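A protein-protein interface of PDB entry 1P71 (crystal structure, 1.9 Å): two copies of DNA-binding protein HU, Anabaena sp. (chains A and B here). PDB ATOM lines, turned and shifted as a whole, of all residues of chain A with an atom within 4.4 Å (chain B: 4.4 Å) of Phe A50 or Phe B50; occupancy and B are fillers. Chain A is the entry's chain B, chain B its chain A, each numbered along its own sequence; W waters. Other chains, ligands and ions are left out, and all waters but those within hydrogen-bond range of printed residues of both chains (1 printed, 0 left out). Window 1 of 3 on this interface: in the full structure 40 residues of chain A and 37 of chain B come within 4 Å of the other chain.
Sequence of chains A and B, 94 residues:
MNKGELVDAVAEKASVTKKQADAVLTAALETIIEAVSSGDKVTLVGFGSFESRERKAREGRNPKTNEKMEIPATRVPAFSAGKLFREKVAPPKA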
ATOM      1  N   ILE A  32     -13.428 -13.756 -23.015  1.00  0.00           N
ATOM      2  CA  ILE A  32     -12.257 -13.026 -23.482  1.00  0.00           C
ATOM      3  C   ILE A  32     -11.057 -13.237 -22.538  1.00  0.00           C
ATOM      4  O   ILE A  32      -9.958 -13.539 -22.997  1.00  0.00           O
ATOM      5  CB  ILE A  32     -12.550 -11.499 -23.676  1.00  0.00           C
ATOM      6  CG1 ILE A  32     -13.389 -11.252 -24.933  1.00  0.00           C
ATOM      7  CG2 ILE A  32     -11.265 -10.767 -23.823  1.00  0.00           C
ATOM      8  CD1 ILE A  32     -14.197  -9.892 -24.925  1.00  0.00           C
ATOM      9  N   VAL A  36      -7.663 -15.083 -23.672  1.00  0.00           N
ATOM     10  CA  VAL A  36      -6.369 -14.397 -23.599  1.00  0.00           C
ATOM     11  C   VAL A  36      -5.394 -15.092 -22.653  1.00  0.00           C
ATOM     12  O   VAL A  36      -4.232 -15.297 -23.007  1.00  0.00           O
ATOM     13  CB  VAL A  36      -6.516 -12.895 -23.248  1.00  0.00           C
ATOM     14  CG1 VAL A  36      -5.150 -12.272 -22.977  1.00  0.00           C
ATOM     15  CG2 VAL A  36      -7.249 -12.170 -24.374  1.00  0.00           C
ATOM     16  N   ASP A  40      -4.707 -17.140 -26.581  1.00  0.00           N
ATOM     17  CA  ASP A  40      -5.508 -16.941 -27.774  1.00  0.00           C
ATOM     18  C   ASP A  40      -5.641 -15.441 -27.970  1.00  0.00           C
ATOM     19  O   ASP A  40      -5.667 -14.676 -26.994  1.00  0.00           O
ATOM     20  CB  ASP A  40      -6.906 -17.562 -27.592  1.00  0.00           C
ATOM     21  CG  ASP A  40      -7.581 -17.964 -28.926  1.00  0.00           C
ATOM     22  OD1 ASP A  40      -8.628 -18.662 -28.883  1.00  0.00           O
ATOM     23  OD2 ASP A  40      -7.145 -17.645 -30.057  1.00  0.00           O
ATOM     24  N   LYS A  41      -5.681 -15.023 -29.231  1.00  0.00           N
ATOM     25  CA  LYS A  41      -6.022 -13.645 -29.579  1.00  0.00           C
ATOM     26  C   LYS A  41      -7.524 -13.555 -29.853  1.00  0.00           C
ATOM     27  O   LYS A  41      -8.070 -14.364 -30.596  1.00  0.00           O
ATOM     28  CB  LYS A  41      -5.208 -13.183 -30.796  1.00  0.00           C
ATOM     29  CG  LYS A  41      -5.436 -11.730 -31.203  1.00  0.00           C
ATOM     30  CD  LYS A  41      -4.797 -11.456 -32.549  1.00  0.00           C
ATOM     31  CE  LYS A  41      -4.343 -10.005 -32.679  1.00  0.00           C
ATOM     32  NZ  LYS A  41      -3.021  -9.890 -33.371  1.00  0.00           N
ATOM     33  N   VAL A  42      -8.179 -12.572 -29.234  1.00  0.00           N
ATOM     34  CA  VAL A  42      -9.594 -12.296 -29.435  1.00  0.00           C
ATOM     35  C   VAL A  42      -9.715 -11.109 -30.399  1.00  0.00           C
ATOM     36  O   VAL A  42      -9.298 -10.003 -30.057  1.00  0.00           O
ATOM     37  CB  VAL A  42     -10.320 -11.998 -28.085  1.00  0.00           C
ATOM     38  CG1 VAL A  42     -11.806 -11.756 -28.305  1.00  0.00           C
ATOM     39  CG2 VAL A  42     -10.143 -13.135 -27.114  1.00  0.00           C
ATOM     40  N   LEU A  44     -12.255  -8.790 -32.690  1.00  0.00           N
ATOM     41  CA  LEU A  44     -13.646  -8.387 -32.880  1.00  0.00           C
ATOM     42  C   LEU A  44     -13.769  -7.308 -33.952  1.00  0.00           C
ATOM     43  O   LEU A  44     -13.454  -6.144 -33.699  1.00  0.00           O
ATOM     44  CB  LEU A  44     -14.257  -7.906 -31.557  1.00  0.00           C
ATOM     45  CG  LEU A  44     -14.001  -8.812 -30.342  1.00  0.00           C
ATOM     46  CD1 LEU A  44     -14.285  -8.079 -29.047  1.00  0.00           C
ATOM     47  CD2 LEU A  44     -14.823 -10.109 -30.415  1.00  0.00           C
ATOM     48  N   PHE A  47     -14.246  -3.343 -33.604  1.00  0.00           N
ATOM     49  CA  PHE A  47     -13.914  -2.889 -32.251  1.00  0.00           C
ATOM     50  C   PHE A  47     -12.395  -2.906 -31.940  1.00  0.00           C
ATOM     51  O   PHE A  47     -11.814  -1.871 -31.621  1.00  0.00           O
ATOM     52  CB  PHE A  47     -14.732  -3.664 -31.216  1.00  0.00           C
ATOM     53  CG  PHE A  47     -14.486  -3.241 -29.787  1.00  0.00           C
ATOM     54  CD1 PHE A  47     -15.087  -2.112 -29.271  1.00  0.00           C
ATOM     55  CD2 PHE A  47     -13.683  -4.014 -28.944  1.00  0.00           C
ATOM     56  CE1 PHE A  47     -14.874  -1.729 -27.938  1.00  0.00           C
ATOM     57  CE2 PHE A  47     -13.464  -3.633 -27.611  1.00  0.00           C
ATOM     58  CZ  PHE A  47     -14.057  -2.479 -27.123  1.00  0.00           C
ATOM     59  N   SER A  49      -8.800  -5.846 -30.872  1.00  0.00           N
ATOM     60  CA  SER A  49      -8.373  -7.183 -30.451  1.00  0.00           C
ATOM     61  C   SER A  49      -7.681  -7.205 -29.084  1.00  0.00           C
ATOM     62  O   SER A  49      -7.103  -6.201 -28.676  1.00  0.00           O
ATOM     63  CB  SER A  49      -7.470  -7.809 -31.516  1.00  0.00           C
ATOM     64  OG  SER A  49      -6.309  -7.041 -31.720  1.00  0.00           O
ATOM     65  N   PHE A  50      -7.782  -8.342 -28.382  1.00  0.00           N
ATOM     66  CA  PHE A  50      -7.129  -8.588 -27.089  1.00  0.00           C
ATOM     67  C   PHE A  50      -6.124  -9.740 -27.202  1.00  0.00           C
ATOM     68  O   PHE A  50      -6.430 -10.801 -27.782  1.00  0.00           O
ATOM     69  CB  PHE A  50      -8.139  -8.954 -25.986  1.00  0.00           C
ATOM     70  CG  PHE A  50      -9.180  -7.916 -25.742  1.00  0.00           C
ATOM     71  CD1 PHE A  50     -10.306  -7.843 -26.554  1.00  0.00           C
ATOM     72  CD2 PHE A  50      -9.035  -6.988 -24.702  1.00  0.00           C
ATOM     73  CE1 PHE A  50     -11.290  -6.860 -26.347  1.00  0.00           C
ATOM     74  CE2 PHE A  50     -10.009  -5.998 -24.500  1.00  0.00           C
ATOM     75  CZ  PHE A  50     -11.128  -5.938 -25.316  1.00  0.00           C
ATOM     76  N   GLU A  51      -4.938  -9.548 -26.635  1.00  0.00           N
ATOM     77  CA  GLU A  51      -3.936 -10.601 -26.647  1.00  0.00           C
ATOM     78  C   GLU A  51      -3.005 -10.519 -25.452  1.00  0.00           C
ATOM     79  O   GLU A  51      -2.950  -9.510 -24.786  1.00  0.00           O
ATOM     80  CB  GLU A  51      -3.122 -10.516 -27.931  1.00  0.00           C
ATOM     81  CG  GLU A  51      -2.097  -9.403 -27.916  1.00  0.00           C
ATOM     82  CD  GLU A  51      -1.492  -9.143 -29.283  1.00  0.00           C
ATOM     83  OE1 GLU A  51      -1.261 -10.102 -30.061  1.00  0.00           O
ATOM     84  OE2 GLU A  51      -1.241  -7.963 -29.577  1.00  0.00           O
ATOM     85  N   ALA A  78      -3.200  -7.068 -23.545  1.00  0.00           N
ATOM     86  CA  ALA A  78      -3.077  -5.839 -24.341  1.00  0.00           C
ATOM     87  C   ALA A  78      -4.252  -5.721 -25.271  1.00  0.00           C
ATOM     88  O   ALA A  78      -4.729  -6.722 -25.786  1.00  0.00           O
ATOM     89  CB  ALA A  78      -1.771  -5.822 -25.136  1.00  0.00           C
ATOM     90  N   PHE A  79      -4.723  -4.496 -25.460  1.00  0.00           N
ATOM     91  CA  PHE A  79      -5.808  -4.204 -26.370  1.00  0.00           C
ATOM     92  C   PHE A  79      -5.264  -3.362 -27.536  1.00  0.00           C
ATOM     93  O   PHE A  79      -4.464  -2.468 -27.323  1.00  0.00           O
ATOM     94  CB  PHE A  79      -6.910  -3.448 -25.616  1.00  0.00           C
ATOM     95  CG  PHE A  79      -8.066  -3.015 -26.480  1.00  0.00           C
ATOM     96  CD1 PHE A  79      -8.888  -3.948 -27.089  1.00  0.00           C
ATOM     97  CD2 PHE A  79      -8.330  -1.657 -26.685  1.00  0.00           C
ATOM     98  CE1 PHE A  79      -9.965  -3.546 -27.892  1.00  0.00           C
ATOM     99  CE2 PHE A  79      -9.386  -1.255 -27.474  1.00  0.00           C
ATOM    100  CZ  PHE A  79     -10.203  -2.193 -28.073  1.00  0.00           C
ATOM    101  N   ILE B  32     -19.515   1.099 -26.190  1.00  0.00           N
ATOM    102  CA  ILE B  32     -18.216   1.424 -25.638  1.00  0.00           C
ATOM    103  C   ILE B  32     -17.503   2.462 -26.509  1.00  0.00           C
ATOM    104  O   ILE B  32     -16.996   3.453 -25.993  1.00  0.00           O
ATOM    105  CB  ILE B  32     -17.337   0.149 -25.486  1.00  0.00           C
ATOM    106  CG1 ILE B  32     -17.886  -0.741 -24.372  1.00  0.00           C
ATOM    107  CG2 ILE B  32     -15.887   0.557 -25.203  1.00  0.00           C
ATOM    108  CD1 ILE B  32     -17.305  -2.196 -24.374  1.00  0.00           C
ATOM    109  N   VAL B  36     -16.538   6.265 -25.235  1.00  0.00           N
ATOM    110  CA  VAL B  36     -15.136   6.683 -25.271  1.00  0.00           C
ATOM    111  C   VAL B  36     -14.935   7.889 -26.211  1.00  0.00           C
ATOM    112  O   VAL B  36     -14.256   8.846 -25.851  1.00  0.00           O
ATOM    113  CB  VAL B  36     -14.193   5.499 -25.584  1.00  0.00           C
ATOM    114  CG1 VAL B  36     -12.740   5.990 -25.929  1.00  0.00           C
ATOM    115  CG2 VAL B  36     -14.184   4.502 -24.412  1.00  0.00           C
ATOM    116  N   ASP B  40     -16.252   9.806 -22.284  1.00  0.00           N
ATOM    117  CA  ASP B  40     -16.547   9.091 -21.056  1.00  0.00           C
ATOM    118  C   ASP B  40     -15.587   7.905 -20.874  1.00  0.00           C
ATOM    119  O   ASP B  40     -15.016   7.395 -21.846  1.00  0.00           O
ATOM    120  CB  ASP B  40     -18.003   8.629 -21.019  1.00  0.00           C
ATOM    121  CG  ASP B  40     -18.518   8.436 -19.591  1.00  0.00           C
ATOM    122  OD1 ASP B  40     -19.614   7.842 -19.433  1.00  0.00           O
ATOM    123  OD2 ASP B  40     -17.905   8.854 -18.568  1.00  0.00           O
ATOM    124  N   LYS B  41     -15.377   7.506 -19.622  1.00  0.00           N
ATOM    125  CA  LYS B  41     -14.583   6.321 -19.304  1.00  0.00           C
ATOM    126  C   LYS B  41     -15.534   5.160 -19.116  1.00  0.00           C
ATOM    127  O   LYS B  41     -16.520   5.288 -18.390  1.00  0.00           O
ATOM    128  CB  LYS B  41     -13.776   6.547 -18.024  1.00  0.00           C
ATOM    129  CG  LYS B  41     -12.754   5.446 -17.678  1.00  0.00           C
ATOM    130  CD  LYS B  41     -11.888   5.919 -16.496  1.00  0.00           C
ATOM    131  CE  LYS B  41     -10.838   4.886 -16.101  1.00  0.00           C
ATOM    132  NZ  LYS B  41      -9.864   5.463 -15.118  1.00  0.00           N
ATOM    133  N   VAL B  42     -15.255   4.032 -19.775  1.00  0.00           N
ATOM    134  CA  VAL B  42     -16.047   2.829 -19.578  1.00  0.00           C
ATOM    135  C   VAL B  42     -15.309   1.926 -18.596  1.00  0.00           C
ATOM    136  O   VAL B  42     -14.163   1.550 -18.808  1.00  0.00           O
ATOM    137  CB  VAL B  42     -16.387   2.071 -20.890  1.00  0.00           C
ATOM    138  CG1 VAL B  42     -17.257   0.835 -20.573  1.00  0.00           C
ATOM    139  CG2 VAL B  42     -17.115   2.964 -21.882  1.00  0.00           C
ATOM    140  N   LEU B  44     -15.308  -1.525 -16.192  1.00  0.00           N
ATOM    141  CA  LEU B  44     -15.886  -2.838 -15.994  1.00  0.00           C
ATOM    142  C   LEU B  44     -15.069  -3.571 -14.938  1.00  0.00           C
ATOM    143  O   LEU B  44     -14.014  -4.093 -15.240  1.00  0.00           O
ATOM    144  CB  LEU B  44     -15.930  -3.604 -17.328  1.00  0.00           C
ATOM    145  CG  LEU B  44     -16.527  -2.871 -18.540  1.00  0.00           C
ATOM    146  CD1 LEU B  44     -16.190  -3.588 -19.831  1.00  0.00           C
ATOM    147  CD2 LEU B  44     -18.058  -2.692 -18.415  1.00  0.00           C
ATOM    148  N   PHE B  47     -12.378  -6.642 -15.209  1.00  0.00           N
ATOM    149  CA  PHE B  47     -11.992  -6.786 -16.605  1.00  0.00           C
ATOM    150  C   PHE B  47     -11.052  -5.669 -17.029  1.00  0.00           C
ATOM    151  O   PHE B  47      -9.928  -5.921 -17.459  1.00  0.00           O
ATOM    152  CB  PHE B  47     -13.220  -6.821 -17.510  1.00  0.00           C
ATOM    153  CG  PHE B  47     -12.883  -6.953 -18.968  1.00  0.00           C
ATOM    154  CD1 PHE B  47     -12.565  -8.203 -19.518  1.00  0.00           C
ATOM    155  CD2 PHE B  47     -12.852  -5.823 -19.787  1.00  0.00           C
ATOM    156  CE1 PHE B  47     -12.241  -8.322 -20.865  1.00  0.00           C
ATOM    157  CE2 PHE B  47     -12.525  -5.921 -21.127  1.00  0.00           C
ATOM    158  CZ  PHE B  47     -12.210  -7.167 -21.672  1.00  0.00           C
ATOM    159  N   SER B  49     -10.786  -1.007 -17.984  1.00  0.00           N
ATOM    160  CA  SER B  49     -11.427   0.243 -18.369  1.00  0.00           C
ATOM    161  C   SER B  49     -10.928   0.710 -19.732  1.00  0.00           C
ATOM    162  O   SER B  49      -9.791   0.429 -20.138  1.00  0.00           O
ATOM    163  CB  SER B  49     -11.159   1.316 -17.326  1.00  0.00           C
ATOM    164  OG  SER B  49      -9.805   1.717 -17.411  1.00  0.00           O
ATOM    165  N   PHE B  50     -11.791   1.454 -20.407  1.00  0.00           N
ATOM    166  CA  PHE B  50     -11.527   2.045 -21.702  1.00  0.00           C
ATOM    167  C   PHE B  50     -11.723   3.550 -21.569  1.00  0.00           C
ATOM    168  O   PHE B  50     -12.696   3.994 -20.963  1.00  0.00           O
ATOM    169  CB  PHE B  50     -12.555   1.565 -22.729  1.00  0.00           C
ATOM    170  CG  PHE B  50     -12.483   0.096 -23.052  1.00  0.00           C
ATOM    171  CD1 PHE B  50     -13.230  -0.821 -22.310  1.00  0.00           C
ATOM    172  CD2 PHE B  50     -11.729  -0.353 -24.138  1.00  0.00           C
ATOM    173  CE1 PHE B  50     -13.206  -2.176 -22.615  1.00  0.00           C
ATOM    174  CE2 PHE B  50     -11.691  -1.711 -24.457  1.00  0.00           C
ATOM    175  CZ  PHE B  50     -12.421  -2.620 -23.695  1.00  0.00           C
ATOM    176  N   GLU B  51     -10.806   4.322 -22.145  1.00  0.00           N
ATOM    177  CA  GLU B  51     -10.920   5.761 -22.132  1.00  0.00           C
ATOM    178  C   GLU B  51     -10.193   6.393 -23.306  1.00  0.00           C
ATOM    179  O   GLU B  51      -9.461   5.732 -24.023  1.00  0.00           O
ATOM    180  CB  GLU B  51     -10.411   6.333 -20.810  1.00  0.00           C
ATOM    181  CG  GLU B  51      -8.966   6.033 -20.484  1.00  0.00           C
ATOM    182  CD  GLU B  51      -8.545   6.721 -19.215  1.00  0.00           C
ATOM    183  OE1 GLU B  51      -9.426   7.227 -18.489  1.00  0.00           O
ATOM    184  OE2 GLU B  51      -7.339   6.778 -18.954  1.00  0.00           O
ATOM    185  N   ALA B  78      -7.786   4.005 -25.121  1.00  0.00           N
ATOM    186  CA  ALA B  78      -6.847   3.282 -24.275  1.00  0.00           C
ATOM    187  C   ALA B  78      -7.568   2.281 -23.374  1.00  0.00           C
ATOM    188  O   ALA B  78      -8.674   2.553 -22.900  1.00  0.00           O
ATOM    189  CB  ALA B  78      -6.031   4.254 -23.458  1.00  0.00           C
ATOM    190  N   PHE B  79      -6.956   1.118 -23.179  1.00  0.00           N
ATOM    191  CA  PHE B  79      -7.490   0.074 -22.307  1.00  0.00           C
ATOM    192  C   PHE B  79      -6.549  -0.145 -21.118  1.00  0.00           C
ATOM    193  O   PHE B  79      -5.341  -0.170 -21.299  1.00  0.00           O
ATOM    194  CB  PHE B  79      -7.667  -1.230 -23.094  1.00  0.00           C
ATOM    195  CG  PHE B  79      -8.155  -2.403 -22.259  1.00  0.00           C
ATOM    196  CD1 PHE B  79      -9.453  -2.437 -21.791  1.00  0.00           C
ATOM    197  CD2 PHE B  79      -7.295  -3.452 -21.930  1.00  0.00           C
ATOM    198  CE1 PHE B  79      -9.921  -3.511 -21.028  1.00  0.00           C
ATOM    199  CE2 PHE B  79      -7.754  -4.536 -21.170  1.00  0.00           C
ATOM    200  CZ  PHE B  79      -9.074  -4.550 -20.717  1.00  0.00           C
ATOM    201  N   PHE B  85      -8.209  -9.731 -14.743  1.00  0.00           N
ATOM    202  CA  PHE B  85      -7.652  -9.978 -16.072  1.00  0.00           C
ATOM    203  C   PHE B  85      -6.115 -10.169 -15.994  1.00  0.00           C
ATOM    204  O   PHE B  85      -5.580 -11.163 -16.477  1.00  0.00           O
ATOM    205  CB  PHE B  85      -8.049  -8.835 -17.006  1.00  0.00           C
ATOM    206  CG  PHE B  85      -7.976  -9.172 -18.471  1.00  0.00           C
ATOM    207  CD1 PHE B  85      -7.325 -10.341 -18.923  1.00  0.00           C
ATOM    208  CD2 PHE B  85      -8.546  -8.326 -19.404  1.00  0.00           C
ATOM    209  CE1 PHE B  85      -7.266 -10.634 -20.274  1.00  0.00           C
ATOM    210  CE2 PHE B  85      -8.492  -8.623 -20.771  1.00  0.00           C
ATOM    211  CZ  PHE B  85      -7.845  -9.777 -21.204  1.00  0.00           C
HETATM  212  O   HOH W   1      -3.796  -2.337 -23.562  1.00  0.00           O
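Water W1 lies within hydrogen-bond range of N of Phe A79 (3.0 Å) and O of Phe B79 (3.5 Å).
Of the printed residues of chain B, Ile A32 touches Phe B47 (3.96 Å). Of the printed residues of chain B, Val A36 touches Phe B85 (3.8 Å). Phe A50 touches just these residues of chain B: Phe B47 and Phe B50. Of the printed residues of chain B, Phe A79 touches Phe B50 and Phe B79. Val B42 touches none of the printed residues of chain A. Of the printed residues of chain A, Phe B47 touches Ile A32 and Phe A50. Ala B78 touches none of the printed residues of chain A. Printed residues of chain A within 4 Å of Phe B85: Val A36. The nearest printed residue of chain B that does not touch Ile A32 is Phe B85 (4.4 Å).
Of the 13 printed residues of chain B, 5 touch a printed residue of chain A. Printed residues of chain B that touch a printed residue of chain A: Ile B32, Phe B47, Phe B50, Phe B79 and Phe B85. Hydrophobic or aromatic side chains of chain B that line the printed part of chain A: Ile B32, Phe B47, Phe B50, Phe B79 and Phe B85. Along chain B the printed residues that touch a printed residue of chain A span positions 32 to 85. Printed residues of chain A that touch a printed residue of chain B: Ile A32, Val A36, Phe A47, Phe A50 and Phe A79. Hydrophobic or aromatic side chains of chain A within 4 Å of the printed part of chain B: Ile A32, Val A36, Phe A47, Phe A50 and Phe A79. Among the printed residues, 8 pairs touch across the chains.
Ile A32 touches Phe B47, and with the chains exchanged Phe A47 touches Ile B32. Phe A50 touches its own counterpart, Phe B50. Phe A79 touches Phe B50, but with the chains exchanged Phe A50 does not touch Phe B79 (4.2 Å). Phe B79 touches its own counterpart, Phe A79.
The backbone carbonyl oxygen (O) of Phe B50 sits at hydrogen-bond distance from the backbone NH (N) of Val B42 (2.8 Å). O of Val A42 sits at hydrogen-bond distance from N of Phe A50, at 2.8 Å.
Among the printed residues, merely in contact across the chains: Phe A79 with Phe B79, Phe A47 with Phe B50, Phe A47 with Ile B32, Phe A50 with Phe B47, Val A36 with Phe B85, Phe A79 with Phe B50, Phe A50 with Phe B50 and Ile A32 with Phe B47.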
